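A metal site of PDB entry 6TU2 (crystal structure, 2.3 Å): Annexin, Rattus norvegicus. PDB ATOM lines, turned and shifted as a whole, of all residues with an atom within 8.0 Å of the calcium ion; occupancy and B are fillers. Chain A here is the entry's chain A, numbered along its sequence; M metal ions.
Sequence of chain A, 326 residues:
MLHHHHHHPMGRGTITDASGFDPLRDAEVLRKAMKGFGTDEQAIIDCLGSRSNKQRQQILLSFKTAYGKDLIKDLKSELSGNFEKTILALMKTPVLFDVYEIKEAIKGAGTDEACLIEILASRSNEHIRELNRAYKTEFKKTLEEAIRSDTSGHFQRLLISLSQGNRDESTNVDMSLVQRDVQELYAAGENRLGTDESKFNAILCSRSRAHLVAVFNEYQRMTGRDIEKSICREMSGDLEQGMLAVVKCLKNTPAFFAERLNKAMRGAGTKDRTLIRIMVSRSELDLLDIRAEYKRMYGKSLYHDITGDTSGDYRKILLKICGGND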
ATOM      1  N   TYR A 186     -11.703 -13.189  27.316  1.00  0.00           N
ATOM      2  CA  TYR A 186     -10.374 -12.592  27.369  1.00  0.00           C
ATOM      3  C   TYR A 186      -9.298 -13.660  27.534  1.00  0.00           C
ATOM      4  O   TYR A 186      -8.250 -13.599  26.891  1.00  0.00           O
ATOM      5  CB  TYR A 186     -10.309 -11.573  28.499  1.00  0.00           C
ATOM      6  CG  TYR A 186      -9.026 -10.765  28.551  1.00  0.00           C
ATOM      7  CD1 TYR A 186      -8.608 -10.021  27.468  1.00  0.00           C
ATOM      8  CD2 TYR A 186      -8.248 -10.741  29.706  1.00  0.00           C
ATOM      9  CE1 TYR A 186      -7.450  -9.282  27.508  1.00  0.00           C
ATOM     10  CE2 TYR A 186      -7.078  -9.996  29.764  1.00  0.00           C
ATOM     11  CZ  TYR A 186      -6.691  -9.266  28.656  1.00  0.00           C
ATOM     12  OH  TYR A 186      -5.530  -8.518  28.691  1.00  0.00           O
ATOM     13  N   ALA A 187      -9.562 -14.653  28.386  1.00  0.00           N
ATOM     14  CA  ALA A 187      -8.585 -15.702  28.645  1.00  0.00           C
ATOM     15  C   ALA A 187      -8.503 -16.720  27.511  1.00  0.00           C
ATOM     16  O   ALA A 187      -7.469 -17.362  27.330  1.00  0.00           O
ATOM     17  CB  ALA A 187      -8.925 -16.423  29.951  1.00  0.00           C
ATOM     18  N   ALA A 188      -9.578 -16.873  26.743  1.00  0.00           N
ATOM     19  CA  ALA A 188      -9.606 -17.879  25.684  1.00  0.00           C
ATOM     20  C   ALA A 188      -8.914 -17.421  24.407  1.00  0.00           C
ATOM     21  O   ALA A 188      -8.683 -18.248  23.520  1.00  0.00           O
ATOM     22  CB  ALA A 188     -11.053 -18.256  25.359  1.00  0.00           C
ATOM     23  N   GLY A 189      -8.579 -16.134  24.278  1.00  0.00           N
ATOM     24  CA  GLY A 189      -7.961 -15.665  23.058  1.00  0.00           C
ATOM     25  C   GLY A 189      -6.915 -14.580  23.250  1.00  0.00           C
ATOM     26  O   GLY A 189      -5.713 -14.829  23.108  1.00  0.00           O
ATOM     27  N   GLU A 190      -7.367 -13.368  23.572  1.00  0.00           N
ATOM     28  CA  GLU A 190      -6.472 -12.205  23.541  1.00  0.00           C
ATOM     29  C   GLU A 190      -5.391 -12.301  24.603  1.00  0.00           C
ATOM     30  O   GLU A 190      -4.247 -11.898  24.356  1.00  0.00           O
ATOM     31  CB  GLU A 190      -7.293 -10.936  23.715  1.00  0.00           C
ATOM     32  CG  GLU A 190      -6.517  -9.650  23.520  1.00  0.00           C
ATOM     33  CD  GLU A 190      -7.258  -8.433  24.022  1.00  0.00           C
ATOM     34  OE1 GLU A 190      -8.508  -8.486  24.088  1.00  0.00           O
ATOM     35  OE2 GLU A 190      -6.595  -7.427  24.371  1.00  0.00           O
ATOM     36  N   ASN A 191      -5.722 -12.815  25.790  1.00  0.00           N
ATOM     37  CA  ASN A 191      -4.778 -12.848  26.913  1.00  0.00           C
ATOM     38  C   ASN A 191      -3.953 -14.122  26.948  1.00  0.00           C
ATOM     39  O   ASN A 191      -3.493 -14.521  28.017  1.00  0.00           O
ATOM     40  CB  ASN A 191      -5.518 -12.662  28.229  1.00  0.00           C
ATOM     41  CG  ASN A 191      -4.595 -12.254  29.369  1.00  0.00           C
ATOM     42  OD1 ASN A 191      -3.610 -11.550  29.163  1.00  0.00           O
ATOM     43  ND2 ASN A 191      -4.911 -12.717  30.569  1.00  0.00           N
ATOM     44  N   ARG A 192      -3.760 -14.783  25.814  1.00  0.00           N
ATOM     45  CA  ARG A 192      -3.005 -16.026  25.793  1.00  0.00           C
ATOM     46  C   ARG A 192      -2.390 -16.215  24.410  1.00  0.00           C
ATOM     47  O   ARG A 192      -2.810 -15.603  23.427  1.00  0.00           O
ATOM     48  CB  ARG A 192      -3.887 -17.230  26.127  1.00  0.00           C
ATOM     49  CG  ARG A 192      -5.091 -17.393  25.209  1.00  0.00           C
ATOM     50  CD  ARG A 192      -5.702 -18.777  25.320  1.00  0.00           C
ATOM     51  NE  ARG A 192      -4.844 -19.794  24.717  1.00  0.00           N
ATOM     52  CZ  ARG A 192      -5.092 -21.092  24.753  1.00  0.00           C
ATOM     53  NH1 ARG A 192      -6.180 -21.555  25.363  1.00  0.00           N
ATOM     54  NH2 ARG A 192      -4.254 -21.950  24.182  1.00  0.00           N
ATOM     55  N   LEU A 193      -1.373 -17.066  24.361  1.00  0.00           N
ATOM     56  CA  LEU A 193      -0.796 -17.493  23.088  1.00  0.00           C
ATOM     57  C   LEU A 193      -1.693 -18.567  22.479  1.00  0.00           C
ATOM     58  O   LEU A 193      -1.962 -19.591  23.120  1.00  0.00           O
ATOM     59  CB  LEU A 193       0.620 -18.005  23.290  1.00  0.00           C
ATOM     60  CG  LEU A 193       1.305 -18.637  22.069  1.00  0.00           C
ATOM     61  CD1 LEU A 193       1.413 -17.636  20.932  1.00  0.00           C
ATOM     62  CD2 LEU A 193       2.670 -19.185  22.454  1.00  0.00           C
ATOM     63  N   GLY A 194      -2.129 -18.341  21.247  1.00  0.00           N
ATOM     64  CA  GLY A 194      -3.079 -19.232  20.627  1.00  0.00           C
ATOM     65  C   GLY A 194      -4.509 -18.861  20.982  1.00  0.00           C
ATOM     66  O   GLY A 194      -4.788 -17.811  21.567  1.00  0.00           O
ATOM     67  N   THR A 195      -5.426 -19.754  20.618  1.00  0.00           N
ATOM     68  CA  THR A 195      -6.848 -19.517  20.782  1.00  0.00           C
ATOM     69  C   THR A 195      -7.536 -20.796  21.222  1.00  0.00           C
ATOM     70  O   THR A 195      -7.241 -21.877  20.702  1.00  0.00           O
ATOM     71  CB  THR A 195      -7.487 -19.012  19.479  1.00  0.00           C
ATOM     72  OG1 THR A 195      -6.733 -17.903  18.976  1.00  0.00           O
ATOM     73  CG2 THR A 195      -8.934 -18.581  19.715  1.00  0.00           C
ATOM     74  N   ASP A 196      -8.455 -20.671  22.177  1.00  0.00           N
ATOM     75  CA  ASP A 196      -9.382 -21.755  22.543  1.00  0.00           C
ATOM     76  C   ASP A 196     -10.709 -21.456  21.848  1.00  0.00           C
ATOM     77  O   ASP A 196     -11.604 -20.833  22.414  1.00  0.00           O
ATOM     78  CB  ASP A 196      -9.554 -21.858  24.053  1.00  0.00           C
ATOM     79  CG  ASP A 196     -10.537 -22.952  24.449  1.00  0.00           C
ATOM     80  OD1 ASP A 196     -10.912 -23.763  23.566  1.00  0.00           O
ATOM     81  OD2 ASP A 196     -10.924 -23.010  25.633  1.00  0.00           O
ATOM     82  N   SER A 230     -11.033  -8.622  18.631  1.00  0.00           N
ATOM     83  CA  SER A 230     -10.389  -9.812  19.189  1.00  0.00           C
ATOM     84  C   SER A 230     -10.624 -11.023  18.291  1.00  0.00           C
ATOM     85  O   SER A 230      -9.701 -11.820  18.060  1.00  0.00           O
ATOM     86  CB  SER A 230     -10.919 -10.087  20.600  1.00  0.00           C
ATOM     87  OG  SER A 230     -10.502  -9.083  21.512  1.00  0.00           O
ATOM     88  N   ARG A 233      -8.461 -10.723  15.364  1.00  0.00           N
ATOM     89  CA  ARG A 233      -7.072 -10.952  15.752  1.00  0.00           C
ATOM     90  C   ARG A 233      -6.806 -12.421  16.009  1.00  0.00           C
ATOM     91  O   ARG A 233      -5.742 -12.949  15.640  1.00  0.00           O
ATOM     92  CB  ARG A 233      -6.728 -10.115  16.985  1.00  0.00           C
ATOM     93  CG  ARG A 233      -5.886  -8.875  16.710  1.00  0.00           C
ATOM     94  CD  ARG A 233      -5.953  -7.882  17.875  1.00  0.00           C
ATOM     95  NE  ARG A 233      -6.774  -6.725  17.546  1.00  0.00           N
ATOM     96  CZ  ARG A 233      -6.341  -5.464  17.504  1.00  0.00           C
ATOM     97  NH1 ARG A 233      -5.084  -5.160  17.805  1.00  0.00           N
ATOM     98  NH2 ARG A 233      -7.184  -4.485  17.188  1.00  0.00           N
ATOM     99  N   GLU A 234      -7.757 -13.123  16.629  1.00  0.00           N
ATOM    100  CA  GLU A 234      -7.532 -14.493  17.055  1.00  0.00           C
ATOM    101  C   GLU A 234      -7.830 -15.522  15.965  1.00  0.00           C
ATOM    102  O   GLU A 234      -7.196 -16.584  15.947  1.00  0.00           O
ATOM    103  CB  GLU A 234      -8.404 -14.816  18.276  1.00  0.00           C
ATOM    104  CG  GLU A 234      -8.019 -14.051  19.537  1.00  0.00           C
ATOM    105  CD  GLU A 234      -6.595 -14.333  19.963  1.00  0.00           C
ATOM    106  OE1 GLU A 234      -5.884 -13.358  20.311  1.00  0.00           O
ATOM    107  OE2 GLU A 234      -6.176 -15.510  19.939  1.00  0.00           O
ATOM    108  N   MET A 235      -8.775 -15.246  15.080  1.00  0.00           N
ATOM    109  CA  MET A 235      -9.251 -16.236  14.131  1.00  0.00           C
ATOM    110  C   MET A 235      -9.081 -15.750  12.700  1.00  0.00           C
ATOM    111  O   MET A 235      -8.978 -14.551  12.430  1.00  0.00           O
ATOM    112  CB  MET A 235     -10.722 -16.575  14.398  1.00  0.00           C
ATOM    113  CG  MET A 235     -10.918 -17.384  15.668  1.00  0.00           C
ATOM    114  SD  MET A 235     -12.559 -17.173  16.391  1.00  0.00           S
ATOM    115  CE  MET A 235     -12.279 -17.848  18.030  1.00  0.00           C
HETATM  116 CA    CA M   1      -3.858 -14.957  21.299  1.00  0.00          CA
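The calcium ion is bound by O of Arg 192, O of Gly 189, OE2 of Glu 234 and OE1 of Glu 234. The calcium ion has four donor atoms within binding distance. Slightly farther from the calcium ion lies O of Gly 194 (3.0 Å).
Within 4 Å of the calcium ion: Gly 189, Arg 192, Gly 194 and Glu 234.
The side-chain hydroxyl of Thr 195 is in hydrogen-bond range of the backbone carbonyl oxygen of Glu 234 (3.3 Å).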
